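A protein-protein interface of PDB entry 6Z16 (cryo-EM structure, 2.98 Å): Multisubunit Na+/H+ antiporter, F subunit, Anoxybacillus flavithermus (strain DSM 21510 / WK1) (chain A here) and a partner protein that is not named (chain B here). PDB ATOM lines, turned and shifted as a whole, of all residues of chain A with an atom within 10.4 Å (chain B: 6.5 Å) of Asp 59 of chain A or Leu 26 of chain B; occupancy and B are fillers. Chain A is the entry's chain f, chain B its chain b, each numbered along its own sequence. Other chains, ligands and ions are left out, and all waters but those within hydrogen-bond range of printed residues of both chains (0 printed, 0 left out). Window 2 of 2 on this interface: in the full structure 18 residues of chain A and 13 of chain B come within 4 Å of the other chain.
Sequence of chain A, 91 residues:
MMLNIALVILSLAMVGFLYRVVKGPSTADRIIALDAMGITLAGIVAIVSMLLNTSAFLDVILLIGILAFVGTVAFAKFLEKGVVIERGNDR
The backbone NH of Gly 36 of chain B lies within hydrogen-bond range of the backbone carbonyl oxygen of Leu 26 of chain B.
Of the 18 printed residues of chain B, 4 touch a printed residue of chain A.
Printed residues of chain B that touch a printed residue of chain A: Phe 22, Leu 26, Pro 34 and Met 43.
Hydrophobic or aromatic side chains of chain B that line the printed part of chain A: Phe 22, Leu 26, Pro 34 and Met 43.
Hydrophobic or aromatic side chains of chain A within 4 Å of the printed part of chain B: Leu 62, Leu 63, Ile 66 and Leu 67.
Among the printed residues, 8 pairs touch across the chains.
Among the printed residues, no Asp or Glu carboxylate lies within 4 Å of a Lys or Arg side-chain nitrogen of the other chain.
Among the printed residues, merely in contact across the chains: Ala 56 of chain A with Pro 34 of chain B (3.8 Å), Asp 59 of chain A with Phe 22 of chain B (3.6 Å), Asp 59 of chain A with Leu 26 of chain B (3.7 Å), Leu 62 of chain A with Phe 22 of chain B (3.6 Å), Leu 63 of chain A with Met 43 of chain B (3.7 Å), Ile 66 of chain A with Phe 22 of chain B (3.7 Å), Ile 66 of chain A with Met 43 of chain B (3.6 Å) and Leu 67 of chain A with Met 43 of chain B (3.7 Å).
Of the printed residues of chain B, Asp 59 of chain A touches Phe 22 (3.6 Å) and Leu 26 (3.7 Å).
Of chain A, only Asp 59 (3.7 Å) comes within 4 Å of Leu 26 of chain B.
No residue of chain A comes within 4 Å of Ala 29 of chain B.
Pro 34 of chain B touches just one residue of chain A: Ala 56 (3.8 Å).
No residue of chain A comes within 4 Å of Gly 35 of chain B.
No residue of chain A comes within 4 Å of Gly 36 of chain B.
Of the printed residues of chain A, Met 43 of chain B touches Leu 63 (3.7 Å), Ile 66 (3.6 Å) and Leu 67 (3.7 Å).
Printed residues of chain B within 4 Å of Leu 63 of chain A: Met 43.
Of the printed residues of chain B, Leu 67 of chain A touches Met 43 (3.7 Å).
Ser 55 of chain A touches none of the printed residues of chain B.
Gly 30 of chain B touches none of the printed residues of chain A.
The nearest residue of chain B that does not touch Asp 59 of chain A is Pro 34 of chain B (4.05 Å).
The nearest residue of chain A that does not touch Leu 26 of chain B is Leu 63 of chain A (5.4 Å).
The nearest printed residue of chain B that does not touch Ala 56 of chain A is Tyr 33 of chain B (7.1 Å).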
ATOM      1  N   ALA A  42      -5.436   0.745  27.806  1.00  0.00           N
ATOM      2  CA  ALA A  42      -4.693   1.847  28.419  1.00  0.00           C
ATOM      3  C   ALA A  42      -4.211   1.484  29.820  1.00  0.00           C
ATOM      4  O   ALA A  42      -3.085   1.827  30.212  1.00  0.00           O
ATOM      5  CB  ALA A  42      -5.556   3.106  28.468  1.00  0.00           C
ATOM      6  N   VAL A  45      -1.227  -0.823  29.459  1.00  0.00           N
ATOM      7  CA  VAL A  45      -0.031  -0.056  29.109  1.00  0.00           C
ATOM      8  C   VAL A  45       0.537   0.653  30.339  1.00  0.00           C
ATOM      9  O   VAL A  45       1.759   0.694  30.530  1.00  0.00           O
ATOM     10  CB  VAL A  45      -0.343   0.920  27.958  1.00  0.00           C
ATOM     11  CG1 VAL A  45       0.823   1.850  27.684  1.00  0.00           C
ATOM     12  CG2 VAL A  45      -0.647   0.148  26.700  1.00  0.00           C
ATOM     13  N   ALA A  46      -0.340   1.153  31.220  1.00  0.00           N
ATOM     14  CA  ALA A  46       0.112   1.774  32.469  1.00  0.00           C
ATOM     15  C   ALA A  46       0.841   0.781  33.374  1.00  0.00           C
ATOM     16  O   ALA A  46       1.919   1.084  33.908  1.00  0.00           O
ATOM     17  CB  ALA A  46      -1.076   2.384  33.209  1.00  0.00           C
ATOM     18  N   SER A  49       4.138  -0.281  31.867  1.00  0.00           N
ATOM     19  CA  SER A  49       5.107   0.798  31.998  1.00  0.00           C
ATOM     20  C   SER A  49       5.656   0.876  33.411  1.00  0.00           C
ATOM     21  O   SER A  49       6.819   1.248  33.601  1.00  0.00           O
ATOM     22  CB  SER A  49       4.473   2.126  31.594  1.00  0.00           C
ATOM     23  OG  SER A  49       3.447   2.487  32.494  1.00  0.00           O
ATOM     24  N   THR A  54       9.943   2.477  33.149  1.00  0.00           N
ATOM     25  CA  THR A  54      10.146   3.565  32.208  1.00  0.00           C
ATOM     26  C   THR A  54       8.963   4.515  32.267  1.00  0.00           C
ATOM     27  O   THR A  54       7.820   4.099  32.466  1.00  0.00           O
ATOM     28  CB  THR A  54      10.314   3.071  30.758  1.00  0.00           C
ATOM     29  OG1 THR A  54       9.126   2.388  30.338  1.00  0.00           O
ATOM     30  CG2 THR A  54      11.509   2.141  30.627  1.00  0.00           C
ATOM     31  N   SER A  55       9.252   5.798  32.077  1.00  0.00           N
ATOM     32  CA  SER A  55       8.230   6.829  31.976  1.00  0.00           C
ATOM     33  C   SER A  55       8.005   7.249  30.528  1.00  0.00           C
ATOM     34  O   SER A  55       7.705   8.412  30.253  1.00  0.00           O
ATOM     35  CB  SER A  55       8.610   8.040  32.824  1.00  0.00           C
ATOM     36  OG  SER A  55       8.699   7.702  34.195  1.00  0.00           O
ATOM     37  N   ALA A  56       8.141   6.314  29.593  1.00  0.00           N
ATOM     38  CA  ALA A  56       8.168   6.636  28.176  1.00  0.00           C
ATOM     39  C   ALA A  56       6.895   6.240  27.443  1.00  0.00           C
ATOM     40  O   ALA A  56       6.867   6.293  26.210  1.00  0.00           O
ATOM     41  CB  ALA A  56       9.374   5.970  27.515  1.00  0.00           C
ATOM     42  N   PHE A  57       5.836   5.854  28.157  1.00  0.00           N
ATOM     43  CA  PHE A  57       4.643   5.339  27.496  1.00  0.00           C
ATOM     44  C   PHE A  57       3.359   5.993  27.997  1.00  0.00           C
ATOM     45  O   PHE A  57       2.277   5.443  27.786  1.00  0.00           O
ATOM     46  CB  PHE A  57       4.542   3.821  27.670  1.00  0.00           C
ATOM     47  CG  PHE A  57       5.646   3.051  26.999  1.00  0.00           C
ATOM     48  CD1 PHE A  57       5.592   2.766  25.644  1.00  0.00           C
ATOM     49  CD2 PHE A  57       6.733   2.601  27.729  1.00  0.00           C
ATOM     50  CE1 PHE A  57       6.604   2.053  25.029  1.00  0.00           C
ATOM     51  CE2 PHE A  57       7.748   1.889  27.120  1.00  0.00           C
ATOM     52  CZ  PHE A  57       7.682   1.614  25.769  1.00  0.00           C
ATOM     53  N   LEU A  58       3.442   7.147  28.660  1.00  0.00           N
ATOM     54  CA  LEU A  58       2.237   7.754  29.220  1.00  0.00           C
ATOM     55  C   LEU A  58       1.450   8.497  28.147  1.00  0.00           C
ATOM     56  O   LEU A  58       0.210   8.614  28.228  1.00  0.00           O
ATOM     57  CB  LEU A  58       2.597   8.708  30.359  1.00  0.00           C
ATOM     58  CG  LEU A  58       3.205   8.145  31.656  1.00  0.00           C
ATOM     59  CD1 LEU A  58       2.537   6.872  32.118  1.00  0.00           C
ATOM     60  CD2 LEU A  58       4.707   7.975  31.617  1.00  0.00           C
ATOM     61  N   ASP A  59       2.169   8.991  27.136  1.00  0.00           N
ATOM     62  CA  ASP A  59       1.545   9.576  25.959  1.00  0.00           C
ATOM     63  C   ASP A  59       0.686   8.560  25.232  1.00  0.00           C
ATOM     64  O   ASP A  59      -0.334   8.924  24.640  1.00  0.00           O
ATOM     65  CB  ASP A  59       2.620  10.118  25.023  1.00  0.00           C
ATOM     66  CG  ASP A  59       3.370  11.291  25.612  1.00  0.00           C
ATOM     67  OD1 ASP A  59       2.766  12.053  26.398  1.00  0.00           O
ATOM     68  OD2 ASP A  59       4.568  11.449  25.294  1.00  0.00           O
ATOM     69  N   VAL A  60       1.070   7.282  25.297  1.00  0.00           N
ATOM     70  CA  VAL A  60       0.254   6.206  24.749  1.00  0.00           C
ATOM     71  C   VAL A  60      -1.071   6.111  25.497  1.00  0.00           C
ATOM     72  O   VAL A  60      -2.119   5.891  24.890  1.00  0.00           O
ATOM     73  CB  VAL A  60       1.039   4.879  24.794  1.00  0.00           C
ATOM     74  CG1 VAL A  60       0.232   3.737  24.218  1.00  0.00           C
ATOM     75  CG2 VAL A  60       2.371   5.017  24.073  1.00  0.00           C
ATOM     76  N   ILE A  61      -1.053   6.344  26.812  1.00  0.00           N
ATOM     77  CA  ILE A  61      -2.270   6.241  27.618  1.00  0.00           C
ATOM     78  C   ILE A  61      -3.247   7.357  27.272  1.00  0.00           C
ATOM     79  O   ILE A  61      -4.436   7.111  27.001  1.00  0.00           O
ATOM     80  CB  ILE A  61      -1.913   6.257  29.113  1.00  0.00           C
ATOM     81  CG1 ILE A  61      -1.064   5.039  29.461  1.00  0.00           C
ATOM     82  CG2 ILE A  61      -3.169   6.325  29.962  1.00  0.00           C
ATOM     83  CD1 ILE A  61      -0.423   5.130  30.797  1.00  0.00           C
ATOM     84  N   LEU A  62      -2.756   8.601  27.252  1.00  0.00           N
ATOM     85  CA  LEU A  62      -3.649   9.705  26.896  1.00  0.00           C
ATOM     86  C   LEU A  62      -4.065   9.644  25.427  1.00  0.00           C
ATOM     87  O   LEU A  62      -5.190  10.043  25.080  1.00  0.00           O
ATOM     88  CB  LEU A  62      -2.994  11.040  27.243  1.00  0.00           C
ATOM     89  CG  LEU A  62      -3.807  12.312  27.001  1.00  0.00           C
ATOM     90  CD1 LEU A  62      -5.154  12.219  27.673  1.00  0.00           C
ATOM     91  CD2 LEU A  62      -3.057  13.504  27.538  1.00  0.00           C
ATOM     92  N   LEU A  63      -3.216   9.059  24.577  1.00  0.00           N
ATOM     93  CA  LEU A  63      -3.562   8.848  23.179  1.00  0.00           C
ATOM     94  C   LEU A  63      -4.681   7.828  23.029  1.00  0.00           C
ATOM     95  O   LEU A  63      -5.592   8.019  22.221  1.00  0.00           O
ATOM     96  CB  LEU A  63      -2.331   8.389  22.409  1.00  0.00           C
ATOM     97  CG  LEU A  63      -2.534   8.357  20.903  1.00  0.00           C
ATOM     98  CD1 LEU A  63      -2.639   9.768  20.390  1.00  0.00           C
ATOM     99  CD2 LEU A  63      -1.422   7.624  20.230  1.00  0.00           C
ATOM    100  N   ILE A  64      -4.617   6.729  23.786  1.00  0.00           N
ATOM    101  CA  ILE A  64      -5.674   5.719  23.755  1.00  0.00           C
ATOM    102  C   ILE A  64      -6.994   6.315  24.228  1.00  0.00           C
ATOM    103  O   ILE A  64      -8.052   6.052  23.637  1.00  0.00           O
ATOM    104  CB  ILE A  64      -5.257   4.490  24.585  1.00  0.00           C
ATOM    105  CG1 ILE A  64      -4.184   3.688  23.858  1.00  0.00           C
ATOM    106  CG2 ILE A  64      -6.420   3.591  24.833  1.00  0.00           C
ATOM    107  CD1 ILE A  64      -3.502   2.693  24.739  1.00  0.00           C
ATOM    108  N   GLY A  65      -6.941   7.182  25.246  1.00  0.00           N
ATOM    109  CA  GLY A  65      -8.158   7.845  25.703  1.00  0.00           C
ATOM    110  C   GLY A  65      -8.789   8.742  24.650  1.00  0.00           C
ATOM    111  O   GLY A  65     -10.002   8.665  24.390  1.00  0.00           O
ATOM    112  N   ILE A  66      -7.970   9.576  23.994  1.00  0.00           N
ATOM    113  CA  ILE A  66      -8.528  10.516  23.020  1.00  0.00           C
ATOM    114  C   ILE A  66      -8.988   9.779  21.759  1.00  0.00           C
ATOM    115  O   ILE A  66     -10.036  10.112  21.188  1.00  0.00           O
ATOM    116  CB  ILE A  66      -7.532  11.669  22.739  1.00  0.00           C
ATOM    117  CG1 ILE A  66      -6.201  11.181  22.188  1.00  0.00           C
ATOM    118  CG2 ILE A  66      -7.220  12.448  24.003  1.00  0.00           C
ATOM    119  CD1 ILE A  66      -5.136  12.273  22.056  1.00  0.00           C
ATOM    120  N   LEU A  67      -8.279   8.708  21.370  1.00  0.00           N
ATOM    121  CA  LEU A  67      -8.694   7.895  20.225  1.00  0.00           C
ATOM    122  C   LEU A  67      -9.991   7.151  20.493  1.00  0.00           C
ATOM    123  O   LEU A  67     -10.845   7.054  19.602  1.00  0.00           O
ATOM    124  CB  LEU A  67      -7.596   6.903  19.850  1.00  0.00           C
ATOM    125  CG  LEU A  67      -6.616   7.237  18.727  1.00  0.00           C
ATOM    126  CD1 LEU A  67      -5.819   8.469  19.008  1.00  0.00           C
ATOM    127  CD2 LEU A  67      -5.681   6.076  18.558  1.00  0.00           C
ATOM    128  N   LEU B  21      -3.340  21.222  23.165  1.00  0.00           N
ATOM    129  CA  LEU B  21      -2.160  21.292  24.030  1.00  0.00           C
ATOM    130  C   LEU B  21      -1.363  19.998  24.009  1.00  0.00           C
ATOM    131  O   LEU B  21      -0.130  20.028  24.043  1.00  0.00           O
ATOM    132  CB  LEU B  21      -2.524  21.617  25.480  1.00  0.00           C
ATOM    133  CG  LEU B  21      -2.519  23.037  26.053  1.00  0.00           C
ATOM    134  CD1 LEU B  21      -3.749  23.818  25.734  1.00  0.00           C
ATOM    135  CD2 LEU B  21      -2.315  22.983  27.548  1.00  0.00           C
ATOM    136  N   PHE B  22      -2.046  18.855  23.930  1.00  0.00           N
ATOM    137  CA  PHE B  22      -1.340  17.581  23.886  1.00  0.00           C
ATOM    138  C   PHE B  22      -0.576  17.411  22.578  1.00  0.00           C
ATOM    139  O   PHE B  22       0.560  16.927  22.582  1.00  0.00           O
ATOM    140  CB  PHE B  22      -2.329  16.440  24.110  1.00  0.00           C
ATOM    141  CG  PHE B  22      -1.707  15.082  24.059  1.00  0.00           C
ATOM    142  CD1 PHE B  22      -0.769  14.703  25.005  1.00  0.00           C
ATOM    143  CD2 PHE B  22      -2.091  14.169  23.094  1.00  0.00           C
ATOM    144  CE1 PHE B  22      -0.200  13.448  24.970  1.00  0.00           C
ATOM    145  CE2 PHE B  22      -1.533  12.912  23.056  1.00  0.00           C
ATOM    146  CZ  PHE B  22      -0.584  12.551  23.994  1.00  0.00           C
ATOM    147  N   SER B  23      -1.160  17.848  21.460  1.00  0.00           N
ATOM    148  CA  SER B  23      -0.475  17.731  20.176  1.00  0.00           C
ATOM    149  C   SER B  23       0.723  18.670  20.091  1.00  0.00           C
ATOM    150  O   SER B  23       1.790  18.278  19.601  1.00  0.00           O
ATOM    151  CB  SER B  23      -1.449  18.001  19.036  1.00  0.00           C
ATOM    152  OG  SER B  23      -1.866  19.350  19.047  1.00  0.00           O
ATOM    153  N   VAL B  24       0.580  19.899  20.593  1.00  0.00           N
ATOM    154  CA  VAL B  24       1.704  20.836  20.581  1.00  0.00           C
ATOM    155  C   VAL B  24       2.799  20.388  21.548  1.00  0.00           C
ATOM    156  O   VAL B  24       3.993  20.535  21.256  1.00  0.00           O
ATOM    157  CB  VAL B  24       1.187  22.258  20.877  1.00  0.00           C
ATOM    158  CG1 VAL B  24       2.313  23.254  21.017  1.00  0.00           C
ATOM    159  CG2 VAL B  24       0.271  22.710  19.761  1.00  0.00           C
ATOM    160  N   GLN B  25       2.425  19.780  22.676  1.00  0.00           N
ATOM    161  CA  GLN B  25       3.424  19.256  23.599  1.00  0.00           C
ATOM    162  C   GLN B  25       4.138  18.035  23.033  1.00  0.00           C
ATOM    163  O   GLN B  25       5.338  17.859  23.276  1.00  0.00           O
ATOM    164  CB  GLN B  25       2.760  18.928  24.935  1.00  0.00           C
ATOM    165  CG  GLN B  25       3.702  18.389  25.993  1.00  0.00           C
ATOM    166  CD  GLN B  25       4.797  19.370  26.342  1.00  0.00           C
ATOM    167  OE1 GLN B  25       4.554  20.570  26.462  1.00  0.00           O
ATOM    168  NE2 GLN B  25       6.012  18.868  26.504  1.00  0.00           N
ATOM    169  N   LEU B  26       3.431  17.197  22.270  1.00  0.00           N
ATOM    170  CA  LEU B  26       4.093  16.110  21.552  1.00  0.00           C
ATOM    171  C   LEU B  26       5.051  16.645  20.502  1.00  0.00           C
ATOM    172  O   LEU B  26       6.124  16.073  20.281  1.00  0.00           O
ATOM    173  CB  LEU B  26       3.067  15.195  20.889  1.00  0.00           C
ATOM    174  CG  LEU B  26       2.263  14.225  21.742  1.00  0.00           C
ATOM    175  CD1 LEU B  26       1.239  13.530  20.874  1.00  0.00           C
ATOM    176  CD2 LEU B  26       3.205  13.228  22.388  1.00  0.00           C
ATOM    177  N   PHE B  27       4.682  17.745  19.849  1.00  0.00           N
ATOM    178  CA  PHE B  27       5.522  18.277  18.785  1.00  0.00           C
ATOM    179  C   PHE B  27       6.787  18.943  19.320  1.00  0.00           C
ATOM    180  O   PHE B  27       7.877  18.713  18.788  1.00  0.00           O
ATOM    181  CB  PHE B  27       4.725  19.250  17.929  1.00  0.00           C
ATOM    182  CG  PHE B  27       5.544  19.925  16.891  1.00  0.00           C
ATOM    183  CD1 PHE B  27       6.046  19.209  15.823  1.00  0.00           C
ATOM    184  CD2 PHE B  27       5.807  21.277  16.975  1.00  0.00           C
ATOM    185  CE1 PHE B  27       6.812  19.830  14.866  1.00  0.00           C
ATOM    186  CE2 PHE B  27       6.570  21.904  16.021  1.00  0.00           C
ATOM    187  CZ  PHE B  27       7.074  21.179  14.966  1.00  0.00           C
ATOM    188  N   PHE B  28       6.670  19.774  20.360  1.00  0.00           N
ATOM    189  CA  PHE B  28       7.833  20.520  20.839  1.00  0.00           C
ATOM    190  C   PHE B  28       8.849  19.651  21.564  1.00  0.00           C
ATOM    191  O   PHE B  28      10.011  20.052  21.676  1.00  0.00           O
ATOM    192  CB  PHE B  28       7.410  21.656  21.771  1.00  0.00           C
ATOM    193  CG  PHE B  28       6.824  22.843  21.067  1.00  0.00           C
ATOM    194  CD1 PHE B  28       7.004  23.022  19.712  1.00  0.00           C
ATOM    195  CD2 PHE B  28       6.100  23.789  21.772  1.00  0.00           C
ATOM    196  CE1 PHE B  28       6.464  24.113  19.066  1.00  0.00           C
ATOM    197  CE2 PHE B  28       5.560  24.884  21.133  1.00  0.00           C
ATOM    198  CZ  PHE B  28       5.741  25.044  19.777  1.00  0.00           C
ATOM    199  N   ALA B  29       8.449  18.486  22.065  1.00  0.00           N
ATOM    200  CA  ALA B  29       9.346  17.605  22.803  1.00  0.00           C
ATOM    201  C   ALA B  29       9.847  16.447  21.955  1.00  0.00           C
ATOM    202  O   ALA B  29      10.085  15.356  22.479  1.00  0.00           O
ATOM    203  CB  ALA B  29       8.653  17.077  24.057  1.00  0.00           C
ATOM    204  N   GLY B  30      10.019  16.664  20.651  1.00  0.00           N
ATOM    205  CA  GLY B  30      10.365  15.566  19.768  1.00  0.00           C
ATOM    206  C   GLY B  30      11.809  15.128  19.893  1.00  0.00           C
ATOM    207  O   GLY B  30      12.103  13.933  19.851  1.00  0.00           O
ATOM    208  N   TYR B  33      12.232  13.557  23.986  1.00  0.00           N
ATOM    209  CA  TYR B  33      11.327  12.552  24.515  1.00  0.00           C
ATOM    210  C   TYR B  33      10.579  11.979  23.318  1.00  0.00           C
ATOM    211  O   TYR B  33      10.745  12.514  22.215  1.00  0.00           O
ATOM    212  CB  TYR B  33      10.426  13.197  25.573  1.00  0.00           C
ATOM    213  CG  TYR B  33      11.230  13.668  26.755  1.00  0.00           C
ATOM    214  CD1 TYR B  33      11.756  12.758  27.660  1.00  0.00           C
ATOM    215  CD2 TYR B  33      11.490  15.016  26.952  1.00  0.00           C
ATOM    216  CE1 TYR B  33      12.512  13.175  28.732  1.00  0.00           C
ATOM    217  CE2 TYR B  33      12.247  15.444  28.025  1.00  0.00           C
ATOM    218  CZ  TYR B  33      12.753  14.519  28.911  1.00  0.00           C
ATOM    219  OH  TYR B  33      13.501  14.940  29.981  1.00  0.00           O
ATOM    220  N   PRO B  34       9.820  10.881  23.441  1.00  0.00           N
ATOM    221  CA  PRO B  34       9.059  10.400  22.283  1.00  0.00           C
ATOM    222  C   PRO B  34       7.985  11.377  21.837  1.00  0.00           C
ATOM    223  O   PRO B  34       7.499  12.204  22.607  1.00  0.00           O
ATOM    224  CB  PRO B  34       8.450   9.084  22.774  1.00  0.00           C
ATOM    225  CG  PRO B  34       8.523   9.139  24.229  1.00  0.00           C
ATOM    226  CD  PRO B  34       9.775   9.884  24.526  1.00  0.00           C
ATOM    227  N   GLY B  35       7.634  11.272  20.565  1.00  0.00           N
ATOM    228  CA  GLY B  35       6.818  12.244  19.874  1.00  0.00           C
ATOM    229  C   GLY B  35       7.556  12.823  18.683  1.00  0.00           C
ATOM    230  O   GLY B  35       8.692  12.461  18.383  1.00  0.00           O
ATOM    231  N   GLY B  36       6.885  13.742  18.004  1.00  0.00           N
ATOM    232  CA  GLY B  36       7.496  14.400  16.865  1.00  0.00           C
ATOM    233  C   GLY B  36       6.439  15.071  16.008  1.00  0.00           C
ATOM    234  O   GLY B  36       5.315  15.291  16.448  1.00  0.00           O
ATOM    235  N   GLY B  37       6.836  15.385  14.773  1.00  0.00           N
ATOM    236  CA  GLY B  37       5.924  16.039  13.854  1.00  0.00           C
ATOM    237  C   GLY B  37       4.795  15.146  13.384  1.00  0.00           C
ATOM    238  O   GLY B  37       3.687  15.632  13.132  1.00  0.00           O
ATOM    239  N   ILE B  39       3.108  12.387  14.957  1.00  0.00           N
ATOM    240  CA  ILE B  39       2.031  12.174  15.913  1.00  0.00           C
ATOM    241  C   ILE B  39       1.385  13.497  16.322  1.00  0.00           C
ATOM    242  O   ILE B  39       0.164  13.560  16.534  1.00  0.00           O
ATOM    243  CB  ILE B  39       2.567  11.360  17.111  1.00  0.00           C
ATOM    244  CG1 ILE B  39       1.433  10.945  18.041  1.00  0.00           C
ATOM    245  CG2 ILE B  39       3.699  12.073  17.840  1.00  0.00           C
ATOM    246  CD1 ILE B  39       0.500   9.986  17.404  1.00  0.00           C
ATOM    247  N   GLY B  40       2.165  14.582  16.360  1.00  0.00           N
ATOM    248  CA  GLY B  40       1.600  15.880  16.681  1.00  0.00           C
ATOM    249  C   GLY B  40       0.684  16.394  15.591  1.00  0.00           C
ATOM    250  O   GLY B  40      -0.391  16.936  15.876  1.00  0.00           O
ATOM    251  N   MET B  43      -2.564  14.326  15.694  1.00  0.00           N
ATOM    252  CA  MET B  43      -3.549  14.654  16.716  1.00  0.00           C
ATOM    253  C   MET B  43      -4.076  16.079  16.639  1.00  0.00           C
ATOM    254  O   MET B  43      -5.187  16.330  17.123  1.00  0.00           O
ATOM    255  CB  MET B  43      -3.014  14.364  18.117  1.00  0.00           C
ATOM    256  CG  MET B  43      -2.747  12.884  18.321  1.00  0.00           C
ATOM    257  SD  MET B  43      -4.013  11.819  17.572  1.00  0.00           S
ATOM    258  CE  MET B  43      -5.535  12.157  18.461  1.00  0.00           C
